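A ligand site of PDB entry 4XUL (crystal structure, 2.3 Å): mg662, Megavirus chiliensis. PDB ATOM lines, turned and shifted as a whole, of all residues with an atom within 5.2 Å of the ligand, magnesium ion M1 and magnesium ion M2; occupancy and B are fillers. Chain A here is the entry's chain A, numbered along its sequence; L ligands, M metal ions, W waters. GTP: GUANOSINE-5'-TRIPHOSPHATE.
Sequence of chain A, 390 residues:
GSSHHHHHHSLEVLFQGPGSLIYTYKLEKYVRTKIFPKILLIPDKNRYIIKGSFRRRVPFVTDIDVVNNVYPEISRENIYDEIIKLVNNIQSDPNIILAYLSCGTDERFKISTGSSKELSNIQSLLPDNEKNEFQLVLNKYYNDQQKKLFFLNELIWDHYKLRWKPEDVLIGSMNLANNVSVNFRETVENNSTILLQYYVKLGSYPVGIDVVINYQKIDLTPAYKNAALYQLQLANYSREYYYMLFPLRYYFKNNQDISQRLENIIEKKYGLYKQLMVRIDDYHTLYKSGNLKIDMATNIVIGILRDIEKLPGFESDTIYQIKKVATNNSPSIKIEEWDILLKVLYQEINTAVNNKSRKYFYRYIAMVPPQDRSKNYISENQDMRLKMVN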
ATOM      1  N   GLY A  52       1.555   7.982 -21.245  1.00  0.00           N
ATOM      2  CA  GLY A  52       0.468   7.350 -21.983  1.00  0.00           C
ATOM      3  C   GLY A  52       0.861   6.872 -23.366  1.00  0.00           C
ATOM      4  O   GLY A  52       2.023   6.603 -23.653  1.00  0.00           O
ATOM      5  N   SER A  53      -0.136   6.778 -24.246  1.00  0.00           N
ATOM      6  CA  SER A  53       0.053   6.165 -25.555  1.00  0.00           C
ATOM      7  C   SER A  53       0.861   7.020 -26.528  1.00  0.00           C
ATOM      8  O   SER A  53       1.457   6.487 -27.463  1.00  0.00           O
ATOM      9  CB  SER A  53      -1.306   5.821 -26.163  1.00  0.00           C
ATOM     10  OG  SER A  53      -2.097   6.988 -26.310  1.00  0.00           O
ATOM     11  N   ARG A  56       4.396   6.199 -26.351  1.00  0.00           N
ATOM     12  CA  ARG A  56       4.682   4.961 -27.052  1.00  0.00           C
ATOM     13  C   ARG A  56       4.501   5.130 -28.559  1.00  0.00           C
ATOM     14  O   ARG A  56       4.672   4.181 -29.327  1.00  0.00           O
ATOM     15  CB  ARG A  56       3.783   3.829 -26.542  1.00  0.00           C
ATOM     16  CG  ARG A  56       4.099   3.366 -25.125  1.00  0.00           C
ATOM     17  CD  ARG A  56       3.403   2.055 -24.809  1.00  0.00           C
ATOM     18  NE  ARG A  56       1.989   2.095 -25.185  1.00  0.00           N
ATOM     19  CZ  ARG A  56       1.030   2.591 -24.413  1.00  0.00           C
ATOM     20  NH1 ARG A  56       1.325   3.082 -23.222  1.00  0.00           N
ATOM     21  NH2 ARG A  56      -0.227   2.589 -24.827  1.00  0.00           N
ATOM     22  N   VAL A  58       1.881   5.455 -30.507  1.00  0.00           N
ATOM     23  CA  VAL A  58       0.902   4.572 -31.131  1.00  0.00           C
ATOM     24  C   VAL A  58       0.334   5.215 -32.398  1.00  0.00           C
ATOM     25  O   VAL A  58       0.147   6.433 -32.451  1.00  0.00           O
ATOM     26  CB  VAL A  58      -0.235   4.196 -30.146  1.00  0.00           C
ATOM     27  CG1 VAL A  58       0.350   3.654 -28.853  1.00  0.00           C
ATOM     28  CG2 VAL A  58      -1.142   5.391 -29.866  1.00  0.00           C
ATOM     29  N   THR A  62      -4.810   9.053 -29.882  1.00  0.00           N
ATOM     30  CA  THR A  62      -6.025   9.274 -29.109  1.00  0.00           C
ATOM     31  C   THR A  62      -5.979  10.642 -28.437  1.00  0.00           C
ATOM     32  O   THR A  62      -6.747  11.535 -28.770  1.00  0.00           O
ATOM     33  CB  THR A  62      -6.219   8.195 -28.038  1.00  0.00           C
ATOM     34  OG1 THR A  62      -5.063   8.141 -27.199  1.00  0.00           O
ATOM     35  CG2 THR A  62      -6.449   6.834 -28.686  1.00  0.00           C
ATOM     36  N   ASP A  63      -5.058  10.787 -27.491  1.00  0.00           N
ATOM     37  CA  ASP A  63      -4.820  12.073 -26.850  1.00  0.00           C
ATOM     38  C   ASP A  63      -3.355  12.191 -26.478  1.00  0.00           C
ATOM     39  O   ASP A  63      -2.562  11.309 -26.780  1.00  0.00           O
ATOM     40  CB  ASP A  63      -5.729  12.243 -25.622  1.00  0.00           C
ATOM     41  CG  ASP A  63      -5.397  11.265 -24.505  1.00  0.00           C
ATOM     42  OD1 ASP A  63      -4.703  10.252 -24.748  1.00  0.00           O
ATOM     43  OD2 ASP A  63      -5.849  11.504 -23.368  1.00  0.00           O
ATOM     44  N   ILE A  64      -3.002  13.287 -25.822  1.00  0.00           N
ATOM     45  CA  ILE A  64      -1.634  13.470 -25.346  1.00  0.00           C
ATOM     46  C   ILE A  64      -1.642  13.758 -23.853  1.00  0.00           C
ATOM     47  O   ILE A  64      -2.318  14.674 -23.392  1.00  0.00           O
ATOM     48  CB  ILE A  64      -0.919  14.616 -26.106  1.00  0.00           C
ATOM     49  CG1 ILE A  64      -0.990  14.392 -27.617  1.00  0.00           C
ATOM     50  CG2 ILE A  64       0.538  14.718 -25.657  1.00  0.00           C
ATOM     51  CD1 ILE A  64      -0.360  15.496 -28.431  1.00  0.00           C
ATOM     52  N   ASP A  65      -0.885  12.955 -23.105  1.00  0.00           N
ATOM     53  CA  ASP A  65      -0.871  13.071 -21.650  1.00  0.00           C
ATOM     54  C   ASP A  65       0.496  13.572 -21.178  1.00  0.00           C
ATOM     55  O   ASP A  65       1.528  12.973 -21.518  1.00  0.00           O
ATOM     56  CB  ASP A  65      -1.218  11.723 -21.010  1.00  0.00           C
ATOM     57  CG  ASP A  65      -2.476  11.101 -21.603  1.00  0.00           C
ATOM     58  OD1 ASP A  65      -3.589  11.466 -21.175  1.00  0.00           O
ATOM     59  OD2 ASP A  65      -2.341  10.240 -22.504  1.00  0.00           O
ATOM     60  N   ASP A 210      -4.131  16.269 -22.035  1.00  0.00           N
ATOM     61  CA  ASP A 210      -4.256  16.297 -20.587  1.00  0.00           C
ATOM     62  C   ASP A 210      -2.924  16.678 -19.940  1.00  0.00           C
ATOM     63  O   ASP A 210      -1.921  15.980 -20.106  1.00  0.00           O
ATOM     64  CB  ASP A 210      -4.721  14.930 -20.058  1.00  0.00           C
ATOM     65  CG  ASP A 210      -6.104  14.551 -20.546  1.00  0.00           C
ATOM     66  OD1 ASP A 210      -6.916  15.462 -20.797  1.00  0.00           O
ATOM     67  OD2 ASP A 210      -6.372  13.340 -20.697  1.00  0.00           O
ATOM     68  N   GLN A 231      -8.531   1.173 -14.063  1.00  0.00           N
ATOM     69  CA  GLN A 231      -8.774   0.781 -15.440  1.00  0.00           C
ATOM     70  C   GLN A 231      -9.050  -0.723 -15.520  1.00  0.00           C
ATOM     71  O   GLN A 231      -9.915  -1.156 -16.287  1.00  0.00           O
ATOM     72  CB  GLN A 231      -7.590   1.175 -16.323  1.00  0.00           C
ATOM     73  CG  GLN A 231      -7.850   1.091 -17.823  1.00  0.00           C
ATOM     74  CD  GLN A 231      -7.678  -0.312 -18.359  1.00  0.00           C
ATOM     75  OE1 GLN A 231      -6.869  -1.085 -17.841  1.00  0.00           O
ATOM     76  NE2 GLN A 231      -8.424  -0.649 -19.402  1.00  0.00           N
ATOM     77  N   LEU A 234     -12.620  -1.206 -14.146  1.00  0.00           N
ATOM     78  CA  LEU A 234     -13.578  -0.684 -15.105  1.00  0.00           C
ATOM     79  C   LEU A 234     -13.803  -1.656 -16.265  1.00  0.00           C
ATOM     80  O   LEU A 234     -14.940  -1.931 -16.645  1.00  0.00           O
ATOM     81  CB  LEU A 234     -13.106   0.663 -15.646  1.00  0.00           C
ATOM     82  CG  LEU A 234     -14.005   1.297 -16.719  1.00  0.00           C
ATOM     83  CD1 LEU A 234     -15.401   1.555 -16.174  1.00  0.00           C
ATOM     84  CD2 LEU A 234     -13.381   2.579 -17.254  1.00  0.00           C
ATOM     85  N   ALA A 235     -12.711  -2.176 -16.804  1.00  0.00           N
ATOM     86  CA  ALA A 235     -12.774  -3.092 -17.941  1.00  0.00           C
ATOM     87  C   ALA A 235     -13.397  -4.425 -17.549  1.00  0.00           C
ATOM     88  O   ALA A 235     -14.272  -4.942 -18.239  1.00  0.00           O
ATOM     89  CB  ALA A 235     -11.384  -3.291 -18.528  1.00  0.00           C
ATOM     90  N   GLU A 240     -15.395  -5.814 -20.751  1.00  0.00           N
ATOM     91  CA  GLU A 240     -14.907  -5.245 -21.996  1.00  0.00           C
ATOM     92  C   GLU A 240     -13.537  -5.840 -22.336  1.00  0.00           C
ATOM     93  O   GLU A 240     -12.504  -5.299 -21.954  1.00  0.00           O
ATOM     94  CB  GLU A 240     -14.844  -3.728 -21.895  1.00  0.00           C
ATOM     95  CG  GLU A 240     -16.212  -3.080 -21.739  1.00  0.00           C
ATOM     96  CD  GLU A 240     -16.133  -1.628 -21.313  1.00  0.00           C
ATOM     97  OE1 GLU A 240     -15.190  -1.279 -20.584  1.00  0.00           O
ATOM     98  OE2 GLU A 240     -17.031  -0.843 -21.689  1.00  0.00           O
ATOM     99  N   TYR A 243     -10.411  -3.776 -23.481  1.00  0.00           N
ATOM    100  CA  TYR A 243      -9.744  -2.992 -22.450  1.00  0.00           C
ATOM    101  C   TYR A 243      -9.168  -3.874 -21.354  1.00  0.00           C
ATOM    102  O   TYR A 243      -8.243  -3.467 -20.655  1.00  0.00           O
ATOM    103  CB  TYR A 243     -10.711  -1.958 -21.885  1.00  0.00           C
ATOM    104  CG  TYR A 243     -11.054  -0.897 -22.910  1.00  0.00           C
ATOM    105  CD1 TYR A 243     -10.099   0.024 -23.314  1.00  0.00           C
ATOM    106  CD2 TYR A 243     -12.319  -0.835 -23.469  1.00  0.00           C
ATOM    107  CE1 TYR A 243     -10.396   0.982 -24.254  1.00  0.00           C
ATOM    108  CE2 TYR A 243     -12.624   0.129 -24.423  1.00  0.00           C
ATOM    109  CZ  TYR A 243     -11.654   1.034 -24.808  1.00  0.00           C
ATOM    110  OH  TYR A 243     -11.939   1.998 -25.752  1.00  0.00           O
ATOM    111  N   PHE A 246      -5.440  -4.372 -21.470  1.00  0.00           N
ATOM    112  CA  PHE A 246      -4.534  -3.330 -20.992  1.00  0.00           C
ATOM    113  C   PHE A 246      -3.721  -3.769 -19.757  1.00  0.00           C
ATOM    114  O   PHE A 246      -2.503  -3.574 -19.743  1.00  0.00           O
ATOM    115  CB  PHE A 246      -5.304  -2.043 -20.672  1.00  0.00           C
ATOM    116  CG  PHE A 246      -5.659  -1.225 -21.887  1.00  0.00           C
ATOM    117  CD1 PHE A 246      -6.211  -1.808 -23.013  1.00  0.00           C
ATOM    118  CD2 PHE A 246      -5.443   0.145 -21.895  1.00  0.00           C
ATOM    119  CE1 PHE A 246      -6.533  -1.047 -24.121  1.00  0.00           C
ATOM    120  CE2 PHE A 246      -5.765   0.911 -22.995  1.00  0.00           C
ATOM    121  CZ  PHE A 246      -6.309   0.317 -24.115  1.00  0.00           C
ATOM    122  N   GLU A 267      -3.068  -1.548 -30.368  1.00  0.00           N
ATOM    123  CA  GLU A 267      -2.824  -0.268 -31.026  1.00  0.00           C
ATOM    124  C   GLU A 267      -2.933  -0.316 -32.548  1.00  0.00           C
ATOM    125  O   GLU A 267      -3.274   0.687 -33.173  1.00  0.00           O
ATOM    126  CB  GLU A 267      -1.457   0.270 -30.618  1.00  0.00           C
ATOM    127  CG  GLU A 267      -1.234   0.379 -29.108  1.00  0.00           C
ATOM    128  CD  GLU A 267      -2.152   1.390 -28.431  1.00  0.00           C
ATOM    129  OE1 GLU A 267      -2.883   2.139 -29.118  1.00  0.00           O
ATOM    130  OE2 GLU A 267      -2.136   1.446 -27.180  1.00  0.00           O
ATOM    131  N   LYS A 274     -10.479   2.040 -30.717  1.00  0.00           N
ATOM    132  CA  LYS A 274     -10.176   2.843 -29.540  1.00  0.00           C
ATOM    133  C   LYS A 274     -10.221   4.329 -29.880  1.00  0.00           C
ATOM    134  O   LYS A 274     -10.808   5.115 -29.142  1.00  0.00           O
ATOM    135  CB  LYS A 274      -8.809   2.457 -28.965  1.00  0.00           C
ATOM    136  CG  LYS A 274      -8.319   3.365 -27.835  1.00  0.00           C
ATOM    137  CD  LYS A 274      -7.236   2.715 -26.961  1.00  0.00           C
ATOM    138  CE  LYS A 274      -6.032   2.255 -27.780  1.00  0.00           C
ATOM    139  NZ  LYS A 274      -5.202   3.390 -28.313  1.00  0.00           N
ATOM    140  N   VAL A 278     -12.645   7.363 -28.330  1.00  0.00           N
ATOM    141  CA  VAL A 278     -12.100   8.587 -27.744  1.00  0.00           C
ATOM    142  C   VAL A 278     -12.656   9.831 -28.441  1.00  0.00           C
ATOM    143  O   VAL A 278     -13.037  10.810 -27.796  1.00  0.00           O
ATOM    144  CB  VAL A 278     -10.563   8.609 -27.796  1.00  0.00           C
ATOM    145  CG1 VAL A 278     -10.023   9.987 -27.446  1.00  0.00           C
ATOM    146  CG2 VAL A 278      -9.989   7.549 -26.868  1.00  0.00           C
ATOM    147  N   ASP A 281     -16.116  10.473 -27.374  1.00  0.00           N
ATOM    148  CA  ASP A 281     -16.101  10.998 -26.014  1.00  0.00           C
ATOM    149  C   ASP A 281     -15.718  12.483 -26.061  1.00  0.00           C
ATOM    150  O   ASP A 281     -16.299  13.295 -25.337  1.00  0.00           O
ATOM    151  CB  ASP A 281     -15.114  10.216 -25.148  1.00  0.00           C
ATOM    152  CG  ASP A 281     -15.809   9.394 -24.083  1.00  0.00           C
ATOM    153  OD1 ASP A 281     -16.886   9.807 -23.613  1.00  0.00           O
ATOM    154  OD2 ASP A 281     -15.269   8.334 -23.703  1.00  0.00           O
ATOM    155  N   TYR A 346     -21.095   4.672 -29.922  1.00  0.00           N
ATOM    156  CA  TYR A 346     -19.987   4.381 -29.029  1.00  0.00           C
ATOM    157  C   TYR A 346     -20.077   2.953 -28.479  1.00  0.00           C
ATOM    158  O   TYR A 346     -19.103   2.216 -28.489  1.00  0.00           O
ATOM    159  CB  TYR A 346     -19.948   5.393 -27.873  1.00  0.00           C
ATOM    160  CG  TYR A 346     -18.849   5.158 -26.851  1.00  0.00           C
ATOM    161  CD1 TYR A 346     -19.001   4.230 -25.825  1.00  0.00           C
ATOM    162  CD2 TYR A 346     -17.668   5.893 -26.897  1.00  0.00           C
ATOM    163  CE1 TYR A 346     -18.013   4.021 -24.891  1.00  0.00           C
ATOM    164  CE2 TYR A 346     -16.668   5.695 -25.959  1.00  0.00           C
ATOM    165  CZ  TYR A 346     -16.841   4.757 -24.960  1.00  0.00           C
ATOM    166  OH  TYR A 346     -15.851   4.557 -24.032  1.00  0.00           O
ATOM    167  N   ASN A 350     -17.827  -0.232 -29.084  1.00  0.00           N
ATOM    168  CA  ASN A 350     -17.318  -0.887 -27.888  1.00  0.00           C
ATOM    169  C   ASN A 350     -17.649  -2.386 -27.891  1.00  0.00           C
ATOM    170  O   ASN A 350     -16.797  -3.227 -27.598  1.00  0.00           O
ATOM    171  CB  ASN A 350     -17.899  -0.206 -26.637  1.00  0.00           C
ATOM    172  CG  ASN A 350     -17.160  -0.590 -25.373  1.00  0.00           C
ATOM    173  OD1 ASN A 350     -15.974  -0.912 -25.397  1.00  0.00           O
ATOM    174  ND2 ASN A 350     -17.860  -0.541 -24.245  1.00  0.00           N
HETATM  175  PG  GTP L   1      -5.163   7.690 -20.726  1.00  0.00           P
HETATM  176  O1G GTP L   1      -5.101   8.694 -21.867  1.00  0.00           O
HETATM  177  O2G GTP L   1      -6.573   7.478 -20.210  1.00  0.00           O
HETATM  178  O3G GTP L   1      -4.132   7.924 -19.649  1.00  0.00           O
HETATM  179  O3B GTP L   1      -4.784   6.256 -21.387  1.00  0.00           O
HETATM  180  PB  GTP L   1      -3.491   5.956 -22.324  1.00  0.00           P
HETATM  181  O1B GTP L   1      -2.897   7.245 -22.861  1.00  0.00           O
HETATM  182  O2B GTP L   1      -2.590   4.999 -21.569  1.00  0.00           O
HETATM  183  O3A GTP L   1      -4.172   5.093 -23.516  1.00  0.00           O
HETATM  184  PA  GTP L   1      -4.956   5.795 -24.739  1.00  0.00           P
HETATM  185  O1A GTP L   1      -4.965   7.289 -24.557  1.00  0.00           O
HETATM  186  O2A GTP L   1      -4.478   5.200 -26.043  1.00  0.00           O
HETATM  187  O5' GTP L   1      -6.444   5.246 -24.465  1.00  0.00           O
HETATM  188  C5' GTP L   1      -7.210   5.885 -23.445  1.00  0.00           C
HETATM  189  C4' GTP L   1      -8.680   5.858 -23.797  1.00  0.00           C
HETATM  190  O4' GTP L   1      -9.185   4.524 -23.778  1.00  0.00           O
HETATM  191  C3' GTP L   1      -9.480   6.644 -22.772  1.00  0.00           C
HETATM  192  O3' GTP L   1      -9.740   7.974 -23.241  1.00  0.00           O
HETATM  193  C2' GTP L   1     -10.784   5.879 -22.640  1.00  0.00           C
HETATM  194  O2' GTP L   1     -11.758   6.540 -23.445  1.00  0.00           O
HETATM  195  C1' GTP L   1     -10.501   4.504 -23.227  1.00  0.00           C
HETATM  196  N9  GTP L   1     -10.597   3.447 -22.182  1.00  0.00           N
HETATM  197  C8  GTP L   1      -9.573   2.981 -21.444  1.00  0.00           C
HETATM  198  N7  GTP L   1      -9.986   2.010 -20.590  1.00  0.00           N
HETATM  199  C5  GTP L   1     -11.311   1.834 -20.791  1.00  0.00           C
HETATM  200  C6  GTP L   1     -12.369   0.960 -20.228  1.00  0.00           C
HETATM  201  O6  GTP L   1     -12.117   0.129 -19.329  1.00  0.00           O
HETATM  202  N1  GTP L   1     -13.616   1.097 -20.702  1.00  0.00           N
HETATM  203  C2  GTP L   1     -13.914   1.982 -21.672  1.00  0.00           C
HETATM  204  N2  GTP L   1     -15.195   2.061 -22.116  1.00  0.00           N
HETATM  205  N3  GTP L   1     -12.997   2.809 -22.230  1.00  0.00           N
HETATM  206  C4  GTP L   1     -11.704   2.782 -21.836  1.00  0.00           C
HETATM  207 MG    MG M   1      -5.593  11.103 -21.341  1.00  0.00          MG
HETATM  208 MG    MG M   2      -3.860   8.942 -23.520  1.00  0.00          MG
HETATM  209  O   HOH W   1      -1.586   8.522 -19.169  1.00  0.00           O
HETATM  210  O   HOH W   2      -7.794   9.255 -23.877  1.00  0.00           O
HETATM  211  O   HOH W   3      -2.556   8.993 -25.152  1.00  0.00           O
HETATM  212  O   HOH W   4      -6.991   4.532 -19.923  1.00  0.00           O
HETATM  213  O   HOH W   5      -3.136   2.650 -25.073  1.00  0.00           O
HETATM  214  O   HOH W   6      -5.650  10.511 -19.310  1.00  0.00           O
HETATM  215  O   HOH W   7      -7.880  10.259 -21.075  1.00  0.00           O
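An oxygen (O2A) of the ligand sits at hydrogen-bond distance from the side-chain hydroxyl (OG) of Ser 53, 3.0 Å away. NZ of Lys 274 is in salt-bridge range of O2A of the ligand, at 3.0 Å. The backbone NH (N) of Ala 235 is in hydrogen-bond range of an oxygen (O6) of the ligand (3.5 Å). OE1 of Glu 240 sits at hydrogen-bond distance from N1 of the ligand (2.9 Å). The side-chain hydroxyl (OG1) of Thr 62 lies within hydrogen-bond range of an oxygen (O2A) of the ligand (3.2 Å). The side-chain hydroxyl (OH) of Tyr 346 sits at hydrogen-bond distance from a nitrogen (N2) of the ligand (3.2 Å). An oxygen (O1B) of the ligand lies close to the backbone NH (N) of Ser 53, at 3.1 Å. NE2 of Gln 231 sits at hydrogen-bond distance from N7 of the ligand.
The side-chain amino group of Lys 274 lies within salt-bridge range of the side-chain carboxylate of Glu 267, at 2.8 Å. The backbone carbonyl oxygen (O) of Ser 53 lies within hydrogen-bond range of the backbone NH (N) of Val 58 (3.2 Å). The side-chain carboxylate (OD1) of Asp 63 lies close to the side-chain hydroxyl (OG1) of Thr 62, at 3.3 Å. N of Asp 210 is in hydrogen-bond range of O of Ile 64 (2.8 Å). The side-chain hydroxyl of Ser 53 is in hydrogen-bond range of the side-chain hydroxyl of Thr 62. The backbone NH of Glu 240 is in hydrogen-bond range of the backbone carbonyl oxygen of Ala 235, 2.9 Å away. The side-chain amide nitrogen of Gln 231 lies within hydrogen-bond range of the backbone carbonyl oxygen of Tyr 243 (3.1 Å). The side-chain amide nitrogen (ND2) of Asn 350 lies within hydrogen-bond range of the side-chain carboxylate (OE2) of Glu 240 (2.7 Å).
Gly 52 touches the ligand. Leu 234 touches the ligand (CG to O6, 3.4 Å). CE1 of Tyr 243 touches N9 of the ligand, at 3.2 Å. CG2 of Val 278 touches O3' of the ligand, 3.7 Å away. Asp 281 touches the ligand (OD2 to O2', 3.95 Å). Hydrophobic or aromatic side chains within 4 Å of the ligand: Leu 234, Ala 235, Tyr 243 and Val 278. The nearest printed residue that does not touch the ligand is Asn 350 (4.3 Å).
The nearest printed residue that does not touch magnesium ion M1 is Ile 64 (5.3 Å).
Residues that only touch magnesium ion M2: Ser 53 (3.8 Å) and Thr 62 (3.95 Å).
OD1 of Asp 65 is bound to magnesium ion M1 (2.0 Å). Magnesium ion M1 is bound by the side-chain carboxylate (OD2) of Asp 63, at 2.1 Å. Water W6 is bound to magnesium ion M1 (2.1 Å). Water W7 is bound to magnesium ion M1 (2.5 Å). OD2 of Asp 210 is bound to magnesium ion M1, 2.5 Å away. An oxygen (O1G) of the ligand is bound to magnesium ion M1 (2.5 Å).
Magnesium ion M2 is bound by the side-chain carboxylate of Asp 63, an oxygen (O1B) of the ligand, an oxygen (O1G) of the ligand, water W3, the side-chain carboxylate of Asp 65 and an oxygen (O1A) of the ligand. Magnesium ion M2 has six donor atoms within binding distance.
Water W3 lies within hydrogen-bond range of the backbone carbonyl oxygen of Asp 63 (2.8 Å), the side-chain hydroxyl of Thr 62 (3.3 Å) and the backbone NH of Ser 53 (3.4 Å). Water W5 lies within hydrogen-bond range of OE2 of Glu 267 (2.6 Å), NH2 of Arg 56 (2.9 Å) and O2A of the ligand (3.0 Å).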
